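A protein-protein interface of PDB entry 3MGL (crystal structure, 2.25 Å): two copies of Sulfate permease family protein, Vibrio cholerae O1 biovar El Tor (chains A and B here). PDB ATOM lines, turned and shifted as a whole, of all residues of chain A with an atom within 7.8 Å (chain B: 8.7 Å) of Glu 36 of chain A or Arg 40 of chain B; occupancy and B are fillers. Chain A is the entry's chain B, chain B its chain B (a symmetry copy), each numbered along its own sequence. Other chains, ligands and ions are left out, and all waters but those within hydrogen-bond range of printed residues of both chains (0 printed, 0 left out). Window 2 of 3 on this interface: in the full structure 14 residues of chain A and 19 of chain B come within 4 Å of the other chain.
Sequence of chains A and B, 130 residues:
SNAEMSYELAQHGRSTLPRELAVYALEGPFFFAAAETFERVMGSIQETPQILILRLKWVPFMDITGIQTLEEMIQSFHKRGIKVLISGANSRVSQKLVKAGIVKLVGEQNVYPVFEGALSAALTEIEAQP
Printed residues of chain A that touch a printed residue of chain B: Phe 32, Ala 33, Glu 36 and Thr 69. Hydrophobic or aromatic side chains of chain A within 4 Å of the printed part of chain B: Phe 32. Printed residues of chain B that touch a printed residue of chain A: Thr 37, Phe 38, Arg 40 and Val 41. Among the printed residues, 6 pairs touch across the chains. Among the printed residues, Asp or Glu carboxylates within 4 Å of a Lys or Arg side-chain nitrogen of the other chain: Glu 36 of chain A with Arg 40 of chain B.
Among the printed residues, pairs that only touch across the chains: Phe 32 of chain A with Phe 38 of chain B (3.4 Å), Glu 36 of chain A with Thr 37 of chain B (3.7 Å), Ala 33 of chain A with Thr 37 of chain B (3.7 Å), Thr 69 of chain A with Val 41 of chain B (3.9 Å) and Phe 32 of chain A with Val 41 of chain B (3.9 Å).
Phe 32 of chain A touches Phe 38 of chain B, but with the chains exchanged Phe 38 of chain A does not touch Phe 32 of chain B (17.2 Å). Phe 32 of chain A touches Val 41 of chain B, but with the chains exchanged Val 41 of chain A does not touch Phe 32 of chain B (20.1 Å). Glu 36 of chain A touches Thr 37 of chain B, but with the chains exchanged Thr 37 of chain A does not touch Glu 36 of chain B (11.0 Å). Glu 36 of chain A touches Arg 40 of chain B, but with the chains exchanged Arg 40 of chain A does not touch Glu 36 of chain B (9.8 Å). Positions printed for both chains: 32, 33, 34, 35, 36, 37, 38, 39, 40, 41, 42 and 73. Of the 6 pairs that touch across the chains among the printed residues, none has its exchanged pair printed and touching as well.
O of Ala 33 of chain A lies within hydrogen-bond range of OG1 of Thr 37 of chain A, 3.0 Å away. NH2 of Arg 40 of chain A lies within salt-bridge range of OE2 of Glu 36 of chain A (3.5 Å). O of Ala 33 of chain B is in hydrogen-bond range of OG1 of Thr 37 of chain B, at 3.0 Å. OE2 of Glu 36 of chain B lies within salt-bridge range of NH2 of Arg 40 of chain B, 3.5 Å away.
The side-chain carboxylate (OE2) of Glu 36 of chain A is in salt-bridge range of the guanidinium group (NH1) of Arg 40 of chain B.
Printed residues of chain B within 4 Å of Phe 32 of chain A: Phe 38 (3.4 Å) and Val 41 (3.9 Å). Of the printed residues of chain B, Ala 33 of chain A touches Thr 37 (3.7 Å). Glu 36 of chain A touches two residues of chain B. Of the printed residues of chain A, Phe 38 of chain B touches Phe 32. Arg 40 of chain B touches one residue of chain A. Gln 46 of chain B touches none of the printed residues of chain A. The nearest printed residue of chain B that does not touch Thr 69 of chain A is Ile 45 of chain B (4.9 Å).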
ATOM      1  N   TYR A  24     -11.738   2.041  -0.628  1.00  0.00           N
ATOM      2  CA  TYR A  24     -12.634   1.046  -1.195  1.00  0.00           C
ATOM      3  C   TYR A  24     -12.016  -0.336  -1.092  1.00  0.00           C
ATOM      4  O   TYR A  24     -10.828  -0.500  -1.335  1.00  0.00           O
ATOM      5  CB  TYR A  24     -12.976   1.371  -2.652  1.00  0.00           C
ATOM      6  CG  TYR A  24     -13.974   0.393  -3.247  1.00  0.00           C
ATOM      7  CD1 TYR A  24     -15.301   0.350  -2.787  1.00  0.00           C
ATOM      8  CD2 TYR A  24     -13.608  -0.480  -4.272  1.00  0.00           C
ATOM      9  CE1 TYR A  24     -16.214  -0.527  -3.313  1.00  0.00           C
ATOM     10  CE2 TYR A  24     -14.539  -1.374  -4.820  1.00  0.00           C
ATOM     11  CZ  TYR A  24     -15.825  -1.387  -4.333  1.00  0.00           C
ATOM     12  OH  TYR A  24     -16.744  -2.269  -4.864  1.00  0.00           O
ATOM     13  N   LEU A  26     -12.104  -4.290  -2.361  1.00  0.00           N
ATOM     14  CA  LEU A  26     -12.515  -5.280  -3.338  1.00  0.00           C
ATOM     15  C   LEU A  26     -13.189  -6.442  -2.627  1.00  0.00           C
ATOM     16  O   LEU A  26     -12.630  -7.028  -1.683  1.00  0.00           O
ATOM     17  CB  LEU A  26     -11.313  -5.740  -4.151  1.00  0.00           C
ATOM     18  CG  LEU A  26     -10.897  -4.768  -5.250  1.00  0.00           C
ATOM     19  CD1 LEU A  26      -9.989  -5.488  -6.266  1.00  0.00           C
ATOM     20  CD2 LEU A  26     -12.160  -4.269  -5.916  1.00  0.00           C
ATOM     21  N   PHE A  31     -15.014  -9.586  -7.461  1.00  0.00           N
ATOM     22  CA  PHE A  31     -15.361  -8.220  -7.145  1.00  0.00           C
ATOM     23  C   PHE A  31     -15.981  -7.469  -8.342  1.00  0.00           C
ATOM     24  O   PHE A  31     -16.236  -6.282  -8.250  1.00  0.00           O
ATOM     25  CB  PHE A  31     -14.101  -7.507  -6.662  1.00  0.00           C
ATOM     26  CG  PHE A  31     -12.942  -7.616  -7.613  1.00  0.00           C
ATOM     27  CD1 PHE A  31     -12.794  -6.715  -8.656  1.00  0.00           C
ATOM     28  CD2 PHE A  31     -11.993  -8.618  -7.454  1.00  0.00           C
ATOM     29  CE1 PHE A  31     -11.710  -6.812  -9.532  1.00  0.00           C
ATOM     30  CE2 PHE A  31     -10.924  -8.724  -8.321  1.00  0.00           C
ATOM     31  CZ  PHE A  31     -10.784  -7.819  -9.368  1.00  0.00           C
ATOM     32  N   PHE A  32     -16.233  -8.175  -9.443  1.00  0.00           N
ATOM     33  CA  PHE A  32     -16.709  -7.572 -10.693  1.00  0.00           C
ATOM     34  C   PHE A  32     -17.936  -6.667 -10.528  1.00  0.00           C
ATOM     35  O   PHE A  32     -17.876  -5.505 -10.903  1.00  0.00           O
ATOM     36  CB  PHE A  32     -17.003  -8.653 -11.750  1.00  0.00           C
ATOM     37  CG  PHE A  32     -15.923  -9.701 -11.883  1.00  0.00           C
ATOM     38  CD1 PHE A  32     -14.653  -9.362 -12.346  1.00  0.00           C
ATOM     39  CD2 PHE A  32     -16.186 -11.023 -11.550  1.00  0.00           C
ATOM     40  CE1 PHE A  32     -13.648 -10.329 -12.473  1.00  0.00           C
ATOM     41  CE2 PHE A  32     -15.199 -12.001 -11.667  1.00  0.00           C
ATOM     42  CZ  PHE A  32     -13.926 -11.661 -12.131  1.00  0.00           C
ATOM     43  N   ALA A  33     -19.033  -7.194  -9.975  1.00  0.00           N
ATOM     44  CA  ALA A  33     -20.265  -6.398  -9.819  1.00  0.00           C
ATOM     45  C   ALA A  33     -20.014  -5.112  -9.024  1.00  0.00           C
ATOM     46  O   ALA A  33     -20.366  -4.024  -9.471  1.00  0.00           O
ATOM     47  CB  ALA A  33     -21.368  -7.213  -9.182  1.00  0.00           C
ATOM     48  N   ALA A  34     -19.368  -5.258  -7.868  1.00  0.00           N
ATOM     49  CA  ALA A  34     -19.100  -4.149  -6.970  1.00  0.00           C
ATOM     50  C   ALA A  34     -18.105  -3.135  -7.555  1.00  0.00           C
ATOM     51  O   ALA A  34     -18.292  -1.931  -7.405  1.00  0.00           O
ATOM     52  CB  ALA A  34     -18.630  -4.674  -5.611  1.00  0.00           C
ATOM     53  N   ALA A  35     -17.062  -3.616  -8.224  1.00  0.00           N
ATOM     54  CA  ALA A  35     -16.133  -2.738  -8.935  1.00  0.00           C
ATOM     55  C   ALA A  35     -16.824  -1.912 -10.036  1.00  0.00           C
ATOM     56  O   ALA A  35     -16.504  -0.746 -10.231  1.00  0.00           O
ATOM     57  CB  ALA A  35     -14.990  -3.543  -9.533  1.00  0.00           C
ATOM     58  N   GLU A  36     -17.771  -2.531 -10.733  1.00  0.00           N
ATOM     59  CA  GLU A  36     -18.504  -1.901 -11.826  1.00  0.00           C
ATOM     60  C   GLU A  36     -19.339  -0.707 -11.318  1.00  0.00           C
ATOM     61  O   GLU A  36     -19.298   0.402 -11.884  1.00  0.00           O
ATOM     62  CB  GLU A  36     -19.368  -2.972 -12.519  1.00  0.00           C
ATOM     63  CG  GLU A  36     -20.221  -2.504 -13.679  1.00  0.00           C
ATOM     64  CD  GLU A  36     -21.034  -3.641 -14.282  1.00  0.00           C
ATOM     65  OE1 GLU A  36     -20.432  -4.676 -14.679  1.00  0.00           O
ATOM     66  OE2 GLU A  36     -22.276  -3.498 -14.355  1.00  0.00           O
ATOM     67  N   THR A  37     -20.056  -0.940 -10.223  1.00  0.00           N
ATOM     68  CA  THR A  37     -20.864   0.087  -9.568  1.00  0.00           C
ATOM     69  C   THR A  37     -20.035   1.281  -9.040  1.00  0.00           C
ATOM     70  O   THR A  37     -20.441   2.438  -9.191  1.00  0.00           O
ATOM     71  CB  THR A  37     -21.728  -0.524  -8.427  1.00  0.00           C
ATOM     72  OG1 THR A  37     -22.221  -1.815  -8.826  1.00  0.00           O
ATOM     73  CG2 THR A  37     -22.916   0.371  -8.134  1.00  0.00           C
ATOM     74  N   PHE A  38     -18.876   0.991  -8.445  1.00  0.00           N
ATOM     75  CA  PHE A  38     -18.022   2.019  -7.849  1.00  0.00           C
ATOM     76  C   PHE A  38     -17.354   2.878  -8.905  1.00  0.00           C
ATOM     77  O   PHE A  38     -17.186   4.077  -8.722  1.00  0.00           O
ATOM     78  CB  PHE A  38     -16.949   1.396  -6.939  1.00  0.00           C
ATOM     79  CG  PHE A  38     -16.211   2.402  -6.109  1.00  0.00           C
ATOM     80  CD1 PHE A  38     -16.896   3.219  -5.198  1.00  0.00           C
ATOM     81  CD2 PHE A  38     -14.836   2.555  -6.235  1.00  0.00           C
ATOM     82  CE1 PHE A  38     -16.205   4.175  -4.415  1.00  0.00           C
ATOM     83  CE2 PHE A  38     -14.152   3.499  -5.457  1.00  0.00           C
ATOM     84  CZ  PHE A  38     -14.838   4.298  -4.550  1.00  0.00           C
ATOM     85  N   GLU A  39     -16.951   2.232  -9.995  1.00  0.00           N
ATOM     86  CA  GLU A  39     -16.475   2.905 -11.194  1.00  0.00           C
ATOM     87  C   GLU A  39     -17.544   3.896 -11.677  1.00  0.00           C
ATOM     88  O   GLU A  39     -17.235   5.054 -11.947  1.00  0.00           O
ATOM     89  CB  GLU A  39     -16.157   1.846 -12.255  1.00  0.00           C
ATOM     90  CG  GLU A  39     -15.116   2.246 -13.267  1.00  0.00           C
ATOM     91  CD  GLU A  39     -14.783   1.117 -14.242  1.00  0.00           C
ATOM     92  OE1 GLU A  39     -14.325   0.035 -13.794  1.00  0.00           O
ATOM     93  OE2 GLU A  39     -14.967   1.320 -15.463  1.00  0.00           O
ATOM     94  N   ARG A  40     -18.803   3.448 -11.720  1.00  0.00           N
ATOM     95  CA  ARG A  40     -19.948   4.285 -12.114  1.00  0.00           C
ATOM     96  C   ARG A  40     -20.132   5.458 -11.153  1.00  0.00           C
ATOM     97  O   ARG A  40     -20.292   6.597 -11.581  1.00  0.00           O
ATOM     98  CB  ARG A  40     -21.233   3.443 -12.207  1.00  0.00           C
ATOM     99  CG  ARG A  40     -22.538   4.226 -12.490  1.00  0.00           C
ATOM    100  CD  ARG A  40     -23.789   3.308 -12.583  1.00  0.00           C
ATOM    101  NE  ARG A  40     -23.465   2.053 -13.263  1.00  0.00           N
ATOM    102  CZ  ARG A  40     -23.469   0.846 -12.692  1.00  0.00           C
ATOM    103  NH1 ARG A  40     -23.830   0.695 -11.421  1.00  0.00           N
ATOM    104  NH2 ARG A  40     -23.127  -0.223 -13.407  1.00  0.00           N
ATOM    105  N   VAL A  41     -20.093   5.179  -9.856  1.00  0.00           N
ATOM    106  CA  VAL A  41     -20.164   6.236  -8.849  1.00  0.00           C
ATOM    107  C   VAL A  41     -19.031   7.246  -9.026  1.00  0.00           C
ATOM    108  O   VAL A  41     -19.272   8.451  -9.083  1.00  0.00           O
ATOM    109  CB  VAL A  41     -20.130   5.668  -7.411  1.00  0.00           C
ATOM    110  CG1 VAL A  41     -19.944   6.783  -6.384  1.00  0.00           C
ATOM    111  CG2 VAL A  41     -21.407   4.850  -7.129  1.00  0.00           C
ATOM    112  N   MET A  42     -17.802   6.755  -9.123  1.00  0.00           N
ATOM    113  CA  MET A  42     -16.658   7.651  -9.256  1.00  0.00           C
ATOM    114  C   MET A  42     -16.785   8.576 -10.471  1.00  0.00           C
ATOM    115  O   MET A  42     -16.550   9.780 -10.365  1.00  0.00           O
ATOM    116  CB  MET A  42     -15.347   6.885  -9.311  1.00  0.00           C
ATOM    117  CG  MET A  42     -14.177   7.762  -8.932  1.00  0.00           C
ATOM    118  SD  MET A  42     -14.276   8.385  -7.069  1.00  0.00           S
ATOM    119  CE  MET A  42     -13.253   6.940  -6.280  1.00  0.00           C
ATOM    120  N   THR A  69     -10.292  -6.230 -15.314  1.00  0.00           N
ATOM    121  CA  THR A  69     -11.292  -5.435 -14.603  1.00  0.00           C
ATOM    122  C   THR A  69     -10.628  -4.362 -13.731  1.00  0.00           C
ATOM    123  O   THR A  69     -11.009  -3.192 -13.771  1.00  0.00           O
ATOM    124  CB  THR A  69     -12.203  -6.329 -13.716  1.00  0.00           C
ATOM    125  OG1 THR A  69     -12.925  -7.281 -14.525  1.00  0.00           O
ATOM    126  CG2 THR A  69     -13.186  -5.484 -12.967  1.00  0.00           C
ATOM    127  N   GLU A  72      -8.872  -1.683 -15.823  1.00  0.00           N
ATOM    128  CA  GLU A  72      -9.871  -0.729 -16.364  1.00  0.00           C
ATOM    129  C   GLU A  72     -10.337   0.238 -15.275  1.00  0.00           C
ATOM    130  O   GLU A  72     -10.470   1.441 -15.510  1.00  0.00           O
ATOM    131  CB  GLU A  72     -11.074  -1.468 -17.012  1.00  0.00           C
ATOM    132  CG  GLU A  72     -12.424  -0.669 -17.084  1.00  0.00           C
ATOM    133  CD  GLU A  72     -13.630  -1.518 -17.566  1.00  0.00           C
ATOM    134  OE1 GLU A  72     -13.610  -2.775 -17.423  1.00  0.00           O
ATOM    135  OE2 GLU A  72     -14.610  -0.919 -18.094  1.00  0.00           O
ATOM    136  N   MET A  73     -10.564  -0.311 -14.085  1.00  0.00           N
ATOM    137  CA  MET A  73     -11.022   0.443 -12.930  1.00  0.00           C
ATOM    138  C   MET A  73     -10.036   1.559 -12.548  1.00  0.00           C
ATOM    139  O   MET A  73     -10.433   2.699 -12.346  1.00  0.00           O
ATOM    140  CB  MET A  73     -11.195  -0.512 -11.752  1.00  0.00           C
ATOM    141  CG  MET A  73     -12.243  -0.092 -10.769  1.00  0.00           C
ATOM    142  SD  MET A  73     -12.085  -0.992  -9.047  1.00  0.00           S
ATOM    143  CE  MET A  73     -13.649  -0.198  -8.254  1.00  0.00           C
ATOM    144  N   PHE B  32     -27.883 -15.997 -10.265  1.00  0.00           N
ATOM    145  CA  PHE B  32     -28.306 -15.230 -11.442  1.00  0.00           C
ATOM    146  C   PHE B  32     -27.604 -13.876 -11.598  1.00  0.00           C
ATOM    147  O   PHE B  32     -26.994 -13.635 -12.630  1.00  0.00           O
ATOM    148  CB  PHE B  32     -29.832 -15.023 -11.445  1.00  0.00           C
ATOM    149  CG  PHE B  32     -30.629 -16.270 -11.138  1.00  0.00           C
ATOM    150  CD1 PHE B  32     -30.611 -17.360 -12.006  1.00  0.00           C
ATOM    151  CD2 PHE B  32     -31.397 -16.343  -9.983  1.00  0.00           C
ATOM    152  CE1 PHE B  32     -31.348 -18.518 -11.727  1.00  0.00           C
ATOM    153  CE2 PHE B  32     -32.136 -17.488  -9.687  1.00  0.00           C
ATOM    154  CZ  PHE B  32     -32.119 -18.579 -10.558  1.00  0.00           C
ATOM    155  N   ALA B  33     -27.689 -13.006 -10.586  1.00  0.00           N
ATOM    156  CA  ALA B  33     -27.073 -11.670 -10.677  1.00  0.00           C
ATOM    157  C   ALA B  33     -25.574 -11.754 -10.985  1.00  0.00           C
ATOM    158  O   ALA B  33     -25.093 -11.120 -11.920  1.00  0.00           O
ATOM    159  CB  ALA B  33     -27.314 -10.867  -9.419  1.00  0.00           C
ATOM    160  N   ALA B  34     -24.865 -12.575 -10.212  1.00  0.00           N
ATOM    161  CA  ALA B  34     -23.426 -12.729 -10.336  1.00  0.00           C
ATOM    162  C   ALA B  34     -23.009 -13.393 -11.658  1.00  0.00           C
ATOM    163  O   ALA B  34     -22.032 -12.978 -12.274  1.00  0.00           O
ATOM    164  CB  ALA B  34     -22.872 -13.489  -9.129  1.00  0.00           C
ATOM    165  N   ALA B  35     -23.749 -14.407 -12.094  1.00  0.00           N
ATOM    166  CA  ALA B  35     -23.522 -15.017 -13.404  1.00  0.00           C
ATOM    167  C   ALA B  35     -23.694 -14.016 -14.562  1.00  0.00           C
ATOM    168  O   ALA B  35     -22.945 -14.052 -15.530  1.00  0.00           O
ATOM    169  CB  ALA B  35     -24.446 -16.207 -13.606  1.00  0.00           C
ATOM    170  N   GLU B  36     -24.678 -13.133 -14.437  1.00  0.00           N
ATOM    171  CA  GLU B  36     -24.992 -12.133 -15.453  1.00  0.00           C
ATOM    172  C   GLU B  36     -23.821 -11.147 -15.642  1.00  0.00           C
ATOM    173  O   GLU B  36     -23.381 -10.870 -16.774  1.00  0.00           O
ATOM    174  CB  GLU B  36     -26.302 -11.425 -15.057  1.00  0.00           C
ATOM    175  CG  GLU B  36     -26.789 -10.336 -15.988  1.00  0.00           C
ATOM    176  CD  GLU B  36     -28.083  -9.703 -15.496  1.00  0.00           C
ATOM    177  OE1 GLU B  36     -29.077 -10.447 -15.271  1.00  0.00           O
ATOM    178  OE2 GLU B  36     -28.104  -8.462 -15.333  1.00  0.00           O
ATOM    179  N   THR B  37     -23.302 -10.659 -14.519  1.00  0.00           N
ATOM    180  CA  THR B  37     -22.154  -9.755 -14.501  1.00  0.00           C
ATOM    181  C   THR B  37     -20.867 -10.380 -15.087  1.00  0.00           C
ATOM    182  O   THR B  37     -20.139  -9.722 -15.838  1.00  0.00           O
ATOM    183  CB  THR B  37     -21.892  -9.213 -13.066  1.00  0.00           C
ATOM    184  OG1 THR B  37     -23.143  -8.952 -12.407  1.00  0.00           O
ATOM    185  CG2 THR B  37     -21.107  -7.917 -13.132  1.00  0.00           C
ATOM    186  N   PHE B  38     -20.609 -11.647 -14.757  1.00  0.00           N
ATOM    187  CA  PHE B  38     -19.397 -12.341 -15.194  1.00  0.00           C
ATOM    188  C   PHE B  38     -19.431 -12.654 -16.677  1.00  0.00           C
ATOM    189  O   PHE B  38     -18.413 -12.589 -17.354  1.00  0.00           O
ATOM    190  CB  PHE B  38     -19.179 -13.641 -14.400  1.00  0.00           C
ATOM    191  CG  PHE B  38     -17.834 -14.260 -14.624  1.00  0.00           C
ATOM    192  CD1 PHE B  38     -16.661 -13.556 -14.315  1.00  0.00           C
ATOM    193  CD2 PHE B  38     -17.721 -15.540 -15.155  1.00  0.00           C
ATOM    194  CE1 PHE B  38     -15.387 -14.134 -14.530  1.00  0.00           C
ATOM    195  CE2 PHE B  38     -16.459 -16.112 -15.362  1.00  0.00           C
ATOM    196  CZ  PHE B  38     -15.302 -15.410 -15.045  1.00  0.00           C
ATOM    197  N   GLU B  39     -20.616 -13.024 -17.155  1.00  0.00           N
ATOM    198  CA  GLU B  39     -20.895 -13.169 -18.576  1.00  0.00           C
ATOM    199  C   GLU B  39     -20.554 -11.858 -19.297  1.00  0.00           C
ATOM    200  O   GLU B  39     -19.861 -11.872 -20.312  1.00  0.00           O
ATOM    201  CB  GLU B  39     -22.370 -13.549 -18.747  1.00  0.00           C
ATOM    202  CG  GLU B  39     -22.690 -14.326 -19.997  1.00  0.00           C
ATOM    203  CD  GLU B  39     -24.158 -14.747 -20.065  1.00  0.00           C
ATOM    204  OE1 GLU B  39     -24.627 -15.483 -19.160  1.00  0.00           O
ATOM    205  OE2 GLU B  39     -24.839 -14.350 -21.036  1.00  0.00           O
ATOM    206  N   ARG B  40     -20.991 -10.729 -18.728  1.00  0.00           N
ATOM    207  CA  ARG B  40     -20.709  -9.388 -19.267  1.00  0.00           C
ATOM    208  C   ARG B  40     -19.209  -9.100 -19.275  1.00  0.00           C
ATOM    209  O   ARG B  40     -18.665  -8.643 -20.276  1.00  0.00           O
ATOM    210  CB  ARG B  40     -21.472  -8.310 -18.477  1.00  0.00           C
ATOM    211  CG  ARG B  40     -21.164  -6.843 -18.861  1.00  0.00           C
ATOM    212  CD  ARG B  40     -21.982  -5.814 -18.030  1.00  0.00           C
ATOM    213  NE  ARG B  40     -23.345  -6.295 -17.800  1.00  0.00           N
ATOM    214  CZ  ARG B  40     -23.853  -6.628 -16.612  1.00  0.00           C
ATOM    215  NH1 ARG B  40     -23.133  -6.494 -15.501  1.00  0.00           N
ATOM    216  NH2 ARG B  40     -25.101  -7.082 -16.532  1.00  0.00           N
ATOM    217  N   VAL B  41     -18.541  -9.383 -18.164  1.00  0.00           N
ATOM    218  CA  VAL B  41     -17.089  -9.235 -18.091  1.00  0.00           C
ATOM    219  C   VAL B  41     -16.391 -10.092 -19.148  1.00  0.00           C
ATOM    220  O   VAL B  41     -15.556  -9.596 -19.901  1.00  0.00           O
ATOM    221  CB  VAL B  41     -16.540  -9.594 -16.690  1.00  0.00           C
ATOM    222  CG1 VAL B  41     -15.015  -9.685 -16.705  1.00  0.00           C
ATOM    223  CG2 VAL B  41     -17.033  -8.573 -15.645  1.00  0.00           C
ATOM    224  N   MET B  42     -16.744 -11.369 -19.209  1.00  0.00           N
ATOM    225  CA  MET B  42     -16.101 -12.267 -20.162  1.00  0.00           C
ATOM    226  C   MET B  42     -16.242 -11.774 -21.606  1.00  0.00           C
ATOM    227  O   MET B  42     -15.267 -11.762 -22.359  1.00  0.00           O
ATOM    228  CB  MET B  42     -16.622 -13.688 -20.037  1.00  0.00           C
ATOM    229  CG  MET B  42     -15.648 -14.689 -20.613  1.00  0.00           C
ATOM    230  SD  MET B  42     -13.943 -14.728 -19.633  1.00  0.00           S
ATOM    231  CE  MET B  42     -14.416 -16.136 -18.388  1.00  0.00           C
ATOM    232  N   GLY B  43     -17.443 -11.321 -21.960  1.00  0.00           N
ATOM    233  CA  GLY B  43     -17.698 -10.744 -23.273  1.00  0.00           C
ATOM    234  C   GLY B  43     -17.127  -9.360 -23.500  1.00  0.00           C
ATOM    235  O   GLY B  43     -17.160  -8.852 -24.627  1.00  0.00           O
ATOM    236  N   SER B  44     -16.588  -8.747 -22.449  1.00  0.00           N
ATOM    237  CA  SER B  44     -16.208  -7.330 -22.506  1.00  0.00           C
ATOM    238  C   SER B  44     -14.696  -7.101 -22.515  1.00  0.00           C
ATOM    239  O   SER B  44     -14.204  -6.147 -23.122  1.00  0.00           O
ATOM    240  CB  SER B  44     -16.863  -6.558 -21.355  1.00  0.00           C
ATOM    241  OG  SER B  44     -16.203  -5.327 -21.130  1.00  0.00           O
ATOM    242  N   ILE B  45     -13.970  -7.976 -21.832  1.00  0.00           N
ATOM    243  CA  ILE B  45     -12.508  -7.913 -21.774  1.00  0.00           C
ATOM    244  C   ILE B  45     -11.862  -8.269 -23.121  1.00  0.00           C
ATOM    245  O   ILE B  45     -12.371  -9.125 -23.847  1.00  0.00           O
ATOM    246  CB  ILE B  45     -11.960  -8.862 -20.680  1.00  0.00           C
ATOM    247  CG1 ILE B  45     -12.459 -10.292 -20.936  1.00  0.00           C
ATOM    248  CG2 ILE B  45     -12.341  -8.312 -19.268  1.00  0.00           C
ATOM    249  CD1 ILE B  45     -11.871 -11.395 -20.020  1.00  0.00           C
ATOM    250  N   GLN B  46     -10.727  -7.633 -23.410  1.00  0.00           N
ATOM    251  CA  GLN B  46      -9.918  -7.893 -24.614  1.00  0.00           C
ATOM    252  C   GLN B  46      -9.430  -9.345 -24.700  1.00  0.00           C
ATOM    253  O   GLN B  46      -9.658 -10.021 -25.707  1.00  0.00           O
ATOM    254  CB  GLN B  46      -8.692  -6.962 -24.669  1.00  0.00           C
ATOM    255  CG  GLN B  46      -8.991  -5.470 -24.804  1.00  0.00           C
ATOM    256  CD  GLN B  46      -7.719  -4.590 -24.957  1.00  0.00           C
ATOM    257  OE1 GLN B  46      -6.579  -5.064 -24.819  1.00  0.00           O
ATOM    258  NE2 GLN B  46      -7.925  -3.304 -25.246  1.00  0.00           N
ATOM    259  N   MET B  73     -24.845 -19.149 -20.082  1.00  0.00           N
ATOM    260  CA  MET B  73     -23.541 -18.713 -19.612  1.00  0.00           C
ATOM    261  C   MET B  73     -22.400 -19.485 -20.294  1.00  0.00           C
ATOM    262  O   MET B  73     -21.447 -18.890 -20.779  1.00  0.00           O
ATOM    263  CB  MET B  73     -23.465 -18.917 -18.101  1.00  0.00           C
ATOM    264  CG  MET B  73     -22.560 -17.955 -17.396  1.00  0.00           C
ATOM    265  SD  MET B  73     -22.058 -18.546 -15.607  1.00  0.00           S
ATOM    266  CE  MET B  73     -21.035 -16.979 -15.152  1.00  0.00           C
ATOM    267  N   SER B  76     -22.038 -18.677 -23.996  1.00  0.00           N
ATOM    268  CA  SER B  76     -21.350 -17.417 -24.252  1.00  0.00           C
ATOM    269  C   SER B  76     -19.835 -17.572 -24.066  1.00  0.00           C
ATOM    270  O   SER B  76     -19.065 -16.942 -24.774  1.00  0.00           O
ATOM    271  CB  SER B  76     -21.937 -16.248 -23.453  1.00  0.00           C
ATOM    272  OG  SER B  76     -21.643 -16.373 -22.084  1.00  0.00           O
ATOM    273  N   PHE B  77     -19.415 -18.465 -23.176  1.00  0.00           N
ATOM    274  CA  PHE B  77     -17.989 -18.778 -23.024  1.00  0.00           C
ATOM    275  C   PHE B  77     -17.422 -19.559 -24.201  1.00  0.00           C
ATOM    276  O   PHE B  77     -16.340 -19.249 -24.669  1.00  0.00           O
ATOM    277  CB  PHE B  77     -17.679 -19.499 -21.683  1.00  0.00           C
ATOM    278  CG  PHE B  77     -18.099 -18.729 -20.466  1.00  0.00           C
ATOM    279  CD1 PHE B  77     -18.185 -17.327 -20.493  1.00  0.00           C
ATOM    280  CD2 PHE B  77     -18.413 -19.391 -19.280  1.00  0.00           C
ATOM    281  CE1 PHE B  77     -18.571 -16.596 -19.358  1.00  0.00           C
ATOM    282  CE2 PHE B  77     -18.795 -18.667 -18.143  1.00  0.00           C
ATOM    283  CZ  PHE B  77     -18.870 -17.258 -18.182  1.00  0.00           C
ATOM    284  N   ARG B  80     -16.529 -17.711 -27.386  1.00  0.00           N
ATOM    285  CA  ARG B  80     -15.247 -16.984 -27.311  1.00  0.00           C
ATOM    286  C   ARG B  80     -13.998 -17.908 -27.268  1.00  0.00           C
ATOM    287  O   ARG B  80     -12.893 -17.453 -26.964  1.00  0.00           O
ATOM    288  CB  ARG B  80     -15.236 -16.020 -26.115  1.00  0.00           C
ATOM    289  CG  ARG B  80     -16.242 -14.851 -26.209  1.00  0.00           C
ATOM    290  CD  ARG B  80     -15.716 -13.558 -25.536  1.00  0.00           C
ATOM    291  NE  ARG B  80     -14.480 -13.046 -26.162  1.00  0.00           N
ATOM    292  CZ  ARG B  80     -13.790 -11.979 -25.755  1.00  0.00           C
ATOM    293  NH1 ARG B  80     -14.180 -11.243 -24.719  1.00  0.00           N
ATOM    294  NH2 ARG B  80     -12.682 -11.654 -26.387  1.00  0.00           N
